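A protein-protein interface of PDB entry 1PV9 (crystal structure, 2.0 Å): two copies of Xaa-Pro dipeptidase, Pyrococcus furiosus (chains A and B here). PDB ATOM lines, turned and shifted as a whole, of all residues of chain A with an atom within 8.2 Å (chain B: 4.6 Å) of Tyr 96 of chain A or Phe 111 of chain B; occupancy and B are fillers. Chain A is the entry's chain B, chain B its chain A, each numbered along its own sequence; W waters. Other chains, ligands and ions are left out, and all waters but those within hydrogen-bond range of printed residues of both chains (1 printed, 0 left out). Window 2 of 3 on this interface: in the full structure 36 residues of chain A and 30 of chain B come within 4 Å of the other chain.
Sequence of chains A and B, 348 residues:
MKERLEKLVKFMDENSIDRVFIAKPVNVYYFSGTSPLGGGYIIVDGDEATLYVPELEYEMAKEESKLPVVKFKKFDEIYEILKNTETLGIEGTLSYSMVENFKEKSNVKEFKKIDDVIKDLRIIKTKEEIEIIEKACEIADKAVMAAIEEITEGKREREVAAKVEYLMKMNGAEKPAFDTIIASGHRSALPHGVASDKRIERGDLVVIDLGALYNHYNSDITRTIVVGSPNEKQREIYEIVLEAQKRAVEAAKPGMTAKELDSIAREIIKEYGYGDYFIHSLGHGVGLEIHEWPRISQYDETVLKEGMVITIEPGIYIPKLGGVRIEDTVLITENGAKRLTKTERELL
N of Tyr 96 of chain A lies within hydrogen-bond range of O of Gly 92 of chain B (3.3 Å). The backbone NH (N) of Tyr 96 of chain A lies within hydrogen-bond range of the backbone carbonyl oxygen (O) of Leu 94 of chain B, 2.8 Å away. The backbone carbonyl oxygen of Gly 92 of chain B lies within hydrogen-bond range of the backbone NH of Ser 97 of chain A (3.0 Å). The backbone carbonyl oxygen of Phe 111 of chain B lies within hydrogen-bond range of the side-chain hydroxyl of Tyr 96 of chain A.
Positions printed for both chains: 92, 94, 99, 102, 103 and 111.
OG of Ser 95 of chain A is in hydrogen-bond range of N of Met 98 of chain A (3.1 Å). N of Ile 90 of chain B sits at hydrogen-bond distance from O of Lys 112 of chain B. The backbone carbonyl oxygen of Ser 97 of chain A lies close to the side-chain amide nitrogen of Asn 101 of chain A (3.4 Å).
Printed residues of chain A that touch a printed residue of chain B: Ser 95, Tyr 96 and Ser 97. Hydrophobic or aromatic side chains of chain A within 4 Å of the printed part of chain B: Tyr 96. Among the printed residues, no Asp or Glu carboxylate lies within 4 Å of a Lys or Arg side-chain nitrogen of the other chain.
Ser 95 of chain A touches Gly 92 of chain B (CB to O, 3.3 Å). Leu 94 of chain B touches Ser 95 of chain A. CD1 of Ile 90 of chain B touches CG of Tyr 96 of chain A (3.6 Å). Val 99 of chain B touches Tyr 96 of chain A (CG2 to CD1, 3.9 Å). Tyr 96 of chain A touches Lys 113 of chain B (CE2 to CG, 3.7 Å). Ser 97 of chain A touches Lys 113 of chain B.
Water W1 bridges the side-chain amino group (NZ) of Lys 103 of chain A (3.2 Å) and the side-chain amino group (NZ) of Lys 103 of chain B (3.2 Å).
Tyr 96 of chain A touches six residues of chain B. Phe 111 of chain B touches just one residue of chain A: Tyr 96 (3.3 Å). Of the printed residues of chain A, Ile 90 of chain B touches Tyr 96. Of the printed residues of chain A, Val 99 of chain B touches Tyr 96. Of the printed residues of chain A, Gly 92 of chain B touches Ser 95 (3.3 Å), Tyr 96 (3.3 Å) and Ser 97 (3.0 Å). Of the printed residues of chain B, Ser 95 of chain A touches Gly 92 (3.3 Å) and Leu 94 (3.6 Å). Met 98 of chain A touches none of the printed residues of chain B. Thr 93 of chain A touches none of the printed residues of chain B. The nearest printed residue of chain B that does not touch Ser 97 of chain A is Leu 94 of chain B (5.1 Å).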
ATOM      1  N   GLY A  92      21.093  -2.654  11.479  1.00  0.00           N
ATOM      2  CA  GLY A  92      20.344  -1.526  10.947  1.00  0.00           C
ATOM      3  C   GLY A  92      19.740  -0.638  12.024  1.00  0.00           C
ATOM      4  O   GLY A  92      19.453   0.535  11.786  1.00  0.00           O
ATOM      5  N   THR A  93      19.563  -1.202  13.215  1.00  0.00           N
ATOM      6  CA  THR A  93      18.994  -0.484  14.351  1.00  0.00           C
ATOM      7  C   THR A  93      20.009   0.409  15.067  1.00  0.00           C
ATOM      8  O   THR A  93      19.626   1.256  15.878  1.00  0.00           O
ATOM      9  CB  THR A  93      18.382  -1.474  15.353  1.00  0.00           C
ATOM     10  OG1 THR A  93      19.262  -2.593  15.517  1.00  0.00           O
ATOM     11  CG2 THR A  93      17.109  -2.091  14.783  1.00  0.00           C
ATOM     12  N   LEU A  94      21.297   0.215  14.776  1.00  0.00           N
ATOM     13  CA  LEU A  94      22.356   1.021  15.386  1.00  0.00           C
ATOM     14  C   LEU A  94      22.051   2.501  15.199  1.00  0.00           C
ATOM     15  O   LEU A  94      21.703   2.933  14.101  1.00  0.00           O
ATOM     16  CB  LEU A  94      23.720   0.686  14.771  1.00  0.00           C
ATOM     17  CG  LEU A  94      24.974   0.468  15.630  1.00  0.00           C
ATOM     18  CD1 LEU A  94      26.192   1.087  14.941  1.00  0.00           C
ATOM     19  CD2 LEU A  94      24.850   0.979  17.064  1.00  0.00           C
ATOM     20  N   SER A  95      22.173   3.269  16.279  1.00  0.00           N
ATOM     21  CA  SER A  95      21.848   4.694  16.260  1.00  0.00           C
ATOM     22  C   SER A  95      22.793   5.504  15.368  1.00  0.00           C
ATOM     23  O   SER A  95      23.972   5.163  15.222  1.00  0.00           O
ATOM     24  CB  SER A  95      21.832   5.258  17.683  1.00  0.00           C
ATOM     25  OG  SER A  95      23.129   5.636  18.114  1.00  0.00           O
ATOM     26  N   TYR A  96      22.257   6.571  14.775  1.00  0.00           N
ATOM     27  CA  TYR A  96      23.032   7.503  13.955  1.00  0.00           C
ATOM     28  C   TYR A  96      24.214   8.074  14.735  1.00  0.00           C
ATOM     29  O   TYR A  96      25.309   8.226  14.189  1.00  0.00           O
ATOM     30  CB  TYR A  96      22.132   8.630  13.441  1.00  0.00           C
ATOM     31  CG  TYR A  96      22.855   9.772  12.755  1.00  0.00           C
ATOM     32  CD1 TYR A  96      23.303   9.653  11.438  1.00  0.00           C
ATOM     33  CD2 TYR A  96      23.074  10.980  13.419  1.00  0.00           C
ATOM     34  CE1 TYR A  96      23.958  10.708  10.803  1.00  0.00           C
ATOM     35  CE2 TYR A  96      23.726  12.038  12.795  1.00  0.00           C
ATOM     36  CZ  TYR A  96      24.161  11.896  11.488  1.00  0.00           C
ATOM     37  OH  TYR A  96      24.810  12.941  10.874  1.00  0.00           O
ATOM     38  N   SER A  97      23.976   8.382  16.009  1.00  0.00           N
ATOM     39  CA  SER A  97      25.010   8.866  16.919  1.00  0.00           C
ATOM     40  C   SER A  97      26.212   7.927  16.952  1.00  0.00           C
ATOM     41  O   SER A  97      27.348   8.371  16.793  1.00  0.00           O
ATOM     42  CB  SER A  97      24.445   9.035  18.332  1.00  0.00           C
ATOM     43  OG  SER A  97      24.013  10.366  18.543  1.00  0.00           O
ATOM     44  N   MET A  98      25.941   6.636  17.138  1.00  0.00           N
ATOM     45  CA  MET A  98      26.980   5.611  17.200  1.00  0.00           C
ATOM     46  C   MET A  98      27.722   5.451  15.877  1.00  0.00           C
ATOM     47  O   MET A  98      28.944   5.313  15.868  1.00  0.00           O
ATOM     48  CB  MET A  98      26.390   4.269  17.635  1.00  0.00           C
ATOM     49  CG  MET A  98      26.285   4.095  19.136  1.00  0.00           C
ATOM     50  SD  MET A  98      27.893   4.143  19.940  1.00  0.00           S
ATOM     51  CE  MET A  98      27.558   5.318  21.252  1.00  0.00           C
ATOM     52  N   VAL A  99      26.978   5.468  14.773  1.00  0.00           N
ATOM     53  CA  VAL A  99      27.567   5.395  13.434  1.00  0.00           C
ATOM     54  C   VAL A  99      28.535   6.561  13.222  1.00  0.00           C
ATOM     55  O   VAL A  99      29.679   6.356  12.803  1.00  0.00           O
ATOM     56  CB  VAL A  99      26.481   5.366  12.323  1.00  0.00           C
ATOM     57  CG1 VAL A  99      27.107   5.451  10.935  1.00  0.00           C
ATOM     58  CG2 VAL A  99      25.632   4.110  12.436  1.00  0.00           C
ATOM     59  N   GLU A 100      28.079   7.772  13.540  1.00  0.00           N
ATOM     60  CA  GLU A 100      28.904   8.975  13.426  1.00  0.00           C
ATOM     61  C   GLU A 100      30.149   8.915  14.308  1.00  0.00           C
ATOM     62  O   GLU A 100      31.223   9.362  13.903  1.00  0.00           O
ATOM     63  CB  GLU A 100      28.090  10.228  13.760  1.00  0.00           C
ATOM     64  CG  GLU A 100      27.142  10.669  12.656  1.00  0.00           C
ATOM     65  CD  GLU A 100      27.858  11.108  11.392  1.00  0.00           C
ATOM     66  OE1 GLU A 100      28.450  12.210  11.389  1.00  0.00           O
ATOM     67  OE2 GLU A 100      27.824  10.350  10.399  1.00  0.00           O
ATOM     68  N   ASN A 101      29.991   8.366  15.512  1.00  0.00           N
ATOM     69  CA  ASN A 101      31.111   8.173  16.429  1.00  0.00           C
ATOM     70  C   ASN A 101      32.141   7.179  15.893  1.00  0.00           C
ATOM     71  O   ASN A 101      33.344   7.383  16.057  1.00  0.00           O
ATOM     72  CB  ASN A 101      30.612   7.736  17.808  1.00  0.00           C
ATOM     73  CG  ASN A 101      30.042   8.888  18.622  1.00  0.00           C
ATOM     74  OD1 ASN A 101      30.354  10.057  18.383  1.00  0.00           O
ATOM     75  ND2 ASN A 101      29.203   8.559  19.597  1.00  0.00           N
ATOM     76  N   PHE A 102      31.665   6.114  15.248  1.00  0.00           N
ATOM     77  CA  PHE A 102      32.549   5.144  14.604  1.00  0.00           C
ATOM     78  C   PHE A 102      33.323   5.771  13.442  1.00  0.00           C
ATOM     79  O   PHE A 102      34.489   5.443  13.220  1.00  0.00           O
ATOM     80  CB  PHE A 102      31.766   3.917  14.127  1.00  0.00           C
ATOM     81  CG  PHE A 102      31.363   2.980  15.236  1.00  0.00           C
ATOM     82  CD1 PHE A 102      32.245   2.680  16.272  1.00  0.00           C
ATOM     83  CD2 PHE A 102      30.102   2.394  15.242  1.00  0.00           C
ATOM     84  CE1 PHE A 102      31.871   1.820  17.301  1.00  0.00           C
ATOM     85  CE2 PHE A 102      29.719   1.529  16.267  1.00  0.00           C
ATOM     86  CZ  PHE A 102      30.606   1.240  17.297  1.00  0.00           C
ATOM     87  N   LYS A 103      32.669   6.674  12.714  1.00  0.00           N
ATOM     88  CA  LYS A 103      33.295   7.380  11.599  1.00  0.00           C
ATOM     89  C   LYS A 103      34.333   8.401  12.068  1.00  0.00           C
ATOM     90  O   LYS A 103      35.408   8.513  11.479  1.00  0.00           O
ATOM     91  CB  LYS A 103      32.233   8.063  10.731  1.00  0.00           C
ATOM     92  CG  LYS A 103      32.038   7.421   9.368  1.00  0.00           C
ATOM     93  CD  LYS A 103      31.257   8.333   8.435  1.00  0.00           C
ATOM     94  CE  LYS A 103      30.064   7.613   7.829  1.00  0.00           C
ATOM     95  NZ  LYS A 103      28.869   8.496   7.738  1.00  0.00           N
ATOM     96  N   PHE A 111      30.159   1.047   6.186  1.00  0.00           N
ATOM     97  CA  PHE A 111      29.293   0.227   7.025  1.00  0.00           C
ATOM     98  C   PHE A 111      28.433  -0.690   6.164  1.00  0.00           C
ATOM     99  O   PHE A 111      27.929  -0.278   5.115  1.00  0.00           O
ATOM    100  CB  PHE A 111      28.399   1.106   7.906  1.00  0.00           C
ATOM    101  CG  PHE A 111      29.158   2.024   8.827  1.00  0.00           C
ATOM    102  CD1 PHE A 111      29.532   1.601  10.100  1.00  0.00           C
ATOM    103  CD2 PHE A 111      29.488   3.317   8.427  1.00  0.00           C
ATOM    104  CE1 PHE A 111      30.231   2.448  10.958  1.00  0.00           C
ATOM    105  CE2 PHE A 111      30.189   4.172   9.277  1.00  0.00           C
ATOM    106  CZ  PHE A 111      30.560   3.736  10.546  1.00  0.00           C
ATOM    107  N   LEU B  88      18.506  17.413   6.644  1.00  0.00           N
ATOM    108  CA  LEU B  88      17.449  16.948   7.534  1.00  0.00           C
ATOM    109  C   LEU B  88      17.953  16.819   8.966  1.00  0.00           C
ATOM    110  O   LEU B  88      18.929  16.113   9.228  1.00  0.00           O
ATOM    111  CB  LEU B  88      16.870  15.616   7.042  1.00  0.00           C
ATOM    112  CG  LEU B  88      15.771  14.951   7.878  1.00  0.00           C
ATOM    113  CD1 LEU B  88      14.423  15.625   7.659  1.00  0.00           C
ATOM    114  CD2 LEU B  88      15.687  13.469   7.553  1.00  0.00           C
ATOM    115  N   ILE B  90      17.767  15.370  12.546  1.00  0.00           N
ATOM    116  CA  ILE B  90      17.293  14.118  13.140  1.00  0.00           C
ATOM    117  C   ILE B  90      17.778  13.946  14.576  1.00  0.00           C
ATOM    118  O   ILE B  90      18.738  14.594  14.997  1.00  0.00           O
ATOM    119  CB  ILE B  90      17.727  12.898  12.279  1.00  0.00           C
ATOM    120  CG1 ILE B  90      19.236  12.926  12.004  1.00  0.00           C
ATOM    121  CG2 ILE B  90      16.928  12.839  10.975  1.00  0.00           C
ATOM    122  CD1 ILE B  90      19.858  11.554  11.841  1.00  0.00           C
ATOM    123  N   GLU B  91      17.103  13.074  15.323  1.00  0.00           N
ATOM    124  CA  GLU B  91      17.569  12.673  16.648  1.00  0.00           C
ATOM    125  C   GLU B  91      18.743  11.712  16.496  1.00  0.00           C
ATOM    126  O   GLU B  91      18.813  10.956  15.522  1.00  0.00           O
ATOM    127  CB  GLU B  91      16.453  12.001  17.453  1.00  0.00           C
ATOM    128  CG  GLU B  91      15.120  12.734  17.432  1.00  0.00           C
ATOM    129  CD  GLU B  91      13.936  11.787  17.521  1.00  0.00           C
ATOM    130  OE1 GLU B  91      13.709  11.015  16.562  1.00  0.00           O
ATOM    131  OE2 GLU B  91      13.235  11.815  18.551  1.00  0.00           O
ATOM    132  N   GLY B  92      19.660  11.741  17.459  1.00  0.00           N
ATOM    133  CA  GLY B  92      20.813  10.854  17.458  1.00  0.00           C
ATOM    134  C   GLY B  92      20.449   9.387  17.625  1.00  0.00           C
ATOM    135  O   GLY B  92      21.228   8.507  17.258  1.00  0.00           O
ATOM    136  N   LEU B  94      17.966   7.969  16.072  1.00  0.00           N
ATOM    137  CA  LEU B  94      17.450   7.484  14.790  1.00  0.00           C
ATOM    138  C   LEU B  94      18.341   6.384  14.226  1.00  0.00           C
ATOM    139  O   LEU B  94      19.566   6.523  14.197  1.00  0.00           O
ATOM    140  CB  LEU B  94      17.323   8.634  13.780  1.00  0.00           C
ATOM    141  CG  LEU B  94      16.105   8.784  12.857  1.00  0.00           C
ATOM    142  CD1 LEU B  94      16.546   8.840  11.398  1.00  0.00           C
ATOM    143  CD2 LEU B  94      15.017   7.719  13.062  1.00  0.00           C
ATOM    144  N   VAL B  99      18.143   6.344   8.428  1.00  0.00           N
ATOM    145  CA  VAL B  99      19.010   7.345   7.803  1.00  0.00           C
ATOM    146  C   VAL B  99      19.298   6.956   6.347  1.00  0.00           C
ATOM    147  O   VAL B  99      19.221   7.799   5.449  1.00  0.00           O
ATOM    148  CB  VAL B  99      20.326   7.554   8.602  1.00  0.00           C
ATOM    149  CG1 VAL B  99      21.252   8.543   7.899  1.00  0.00           C
ATOM    150  CG2 VAL B  99      20.023   8.034  10.019  1.00  0.00           C
ATOM    151  N   PHE B 102      16.231   7.531   4.234  1.00  0.00           N
ATOM    152  CA  PHE B 102      16.092   8.937   3.867  1.00  0.00           C
ATOM    153  C   PHE B 102      17.031   9.319   2.722  1.00  0.00           C
ATOM    154  O   PHE B 102      16.711  10.197   1.918  1.00  0.00           O
ATOM    155  CB  PHE B 102      16.339   9.842   5.078  1.00  0.00           C
ATOM    156  CG  PHE B 102      15.169   9.938   6.023  1.00  0.00           C
ATOM    157  CD1 PHE B 102      13.877  10.153   5.545  1.00  0.00           C
ATOM    158  CD2 PHE B 102      15.362   9.822   7.396  1.00  0.00           C
ATOM    159  CE1 PHE B 102      12.798  10.242   6.418  1.00  0.00           C
ATOM    160  CE2 PHE B 102      14.289   9.913   8.280  1.00  0.00           C
ATOM    161  CZ  PHE B 102      13.004  10.125   7.790  1.00  0.00           C
ATOM    162  N   LYS B 103      18.185   8.654   2.655  1.00  0.00           N
ATOM    163  CA  LYS B 103      19.151   8.861   1.576  1.00  0.00           C
ATOM    164  C   LYS B 103      18.613   8.366   0.233  1.00  0.00           C
ATOM    165  O   LYS B 103      18.738   9.052  -0.783  1.00  0.00           O
ATOM    166  CB  LYS B 103      20.471   8.151   1.889  1.00  0.00           C
ATOM    167  CG  LYS B 103      21.370   8.885   2.864  1.00  0.00           C
ATOM    168  CD  LYS B 103      22.326   7.922   3.548  1.00  0.00           C
ATOM    169  CE  LYS B 103      23.482   8.656   4.204  1.00  0.00           C
ATOM    170  NZ  LYS B 103      24.697   7.799   4.307  1.00  0.00           N
ATOM    171  N   VAL B 108      17.823  12.839   0.635  1.00  0.00           N
ATOM    172  CA  VAL B 108      18.428  13.757   1.592  1.00  0.00           C
ATOM    173  C   VAL B 108      19.946  13.768   1.408  1.00  0.00           C
ATOM    174  O   VAL B 108      20.581  12.712   1.363  1.00  0.00           O
ATOM    175  CB  VAL B 108      18.051  13.393   3.056  1.00  0.00           C
ATOM    176  CG1 VAL B 108      18.669  14.373   4.039  1.00  0.00           C
ATOM    177  CG2 VAL B 108      16.535  13.363   3.230  1.00  0.00           C
ATOM    178  N   GLU B 110      22.196  15.709   3.384  1.00  0.00           N
ATOM    179  CA  GLU B 110      22.917  15.889   4.646  1.00  0.00           C
ATOM    180  C   GLU B 110      22.032  15.675   5.873  1.00  0.00           C
ATOM    181  O   GLU B 110      20.837  15.975   5.850  1.00  0.00           O
ATOM    182  CB  GLU B 110      23.562  17.278   4.705  1.00  0.00           C
ATOM    183  CG  GLU B 110      24.933  17.303   5.362  1.00  0.00           C
ATOM    184  CD  GLU B 110      25.630  18.639   5.205  1.00  0.00           C
ATOM    185  OE1 GLU B 110      25.360  19.552   6.013  1.00  0.00           O
ATOM    186  OE2 GLU B 110      26.450  18.778   4.272  1.00  0.00           O
ATOM    187  N   PHE B 111      22.635  15.159   6.942  1.00  0.00           N
ATOM    188  CA  PHE B 111      21.941  14.938   8.208  1.00  0.00           C
ATOM    189  C   PHE B 111      22.650  15.673   9.338  1.00  0.00           C
ATOM    190  O   PHE B 111      23.883  15.711   9.385  1.00  0.00           O
ATOM    191  CB  PHE B 111      21.848  13.442   8.528  1.00  0.00           C
ATOM    192  CG  PHE B 111      21.090  12.646   7.501  1.00  0.00           C
ATOM    193  CD1 PHE B 111      21.751  12.078   6.414  1.00  0.00           C
ATOM    194  CD2 PHE B 111      19.713  12.465   7.618  1.00  0.00           C
ATOM    195  CE1 PHE B 111      21.054  11.346   5.456  1.00  0.00           C
ATOM    196  CE2 PHE B 111      19.008  11.733   6.668  1.00  0.00           C
ATOM    197  CZ  PHE B 111      19.681  11.170   5.585  1.00  0.00           C
ATOM    198  N   LYS B 112      21.864  16.258  10.239  1.00  0.00           N
ATOM    199  CA  LYS B 112      22.401  16.985  11.389  1.00  0.00           C
ATOM    200  C   LYS B 112      21.622  16.645  12.656  1.00  0.00           C
ATOM    201  O   LYS B 112      20.399  16.507  12.621  1.00  0.00           O
ATOM    202  CB  LYS B 112      22.375  18.495  11.131  1.00  0.00           C
ATOM    203  CG  LYS B 112      23.506  18.991  10.233  1.00  0.00           C
ATOM    204  CD  LYS B 112      23.564  20.509  10.173  1.00  0.00           C
ATOM    205  CE  LYS B 112      24.445  20.978   9.025  1.00  0.00           C
ATOM    206  NZ  LYS B 112      24.894  22.388   9.192  1.00  0.00           N
ATOM    207  N   LYS B 113      22.337  16.506  13.769  1.00  0.00           N
ATOM    208  CA  LYS B 113      21.715  16.154  15.044  1.00  0.00           C
ATOM    209  C   LYS B 113      21.008  17.344  15.685  1.00  0.00           C
ATOM    210  O   LYS B 113      21.491  18.476  15.615  1.00  0.00           O
ATOM    211  CB  LYS B 113      22.745  15.568  16.012  1.00  0.00           C
ATOM    212  CG  LYS B 113      23.074  14.103  15.758  1.00  0.00           C
ATOM    213  CD  LYS B 113      23.592  13.408  17.014  1.00  0.00           C
ATOM    214  CE  LYS B 113      25.115  13.449  17.118  1.00  0.00           C
ATOM    215  NZ  LYS B 113      25.799  13.047  15.853  1.00  0.00           N
HETATM  216  O   HOH W   1      26.830   6.445   6.328  1.00  0.00           O
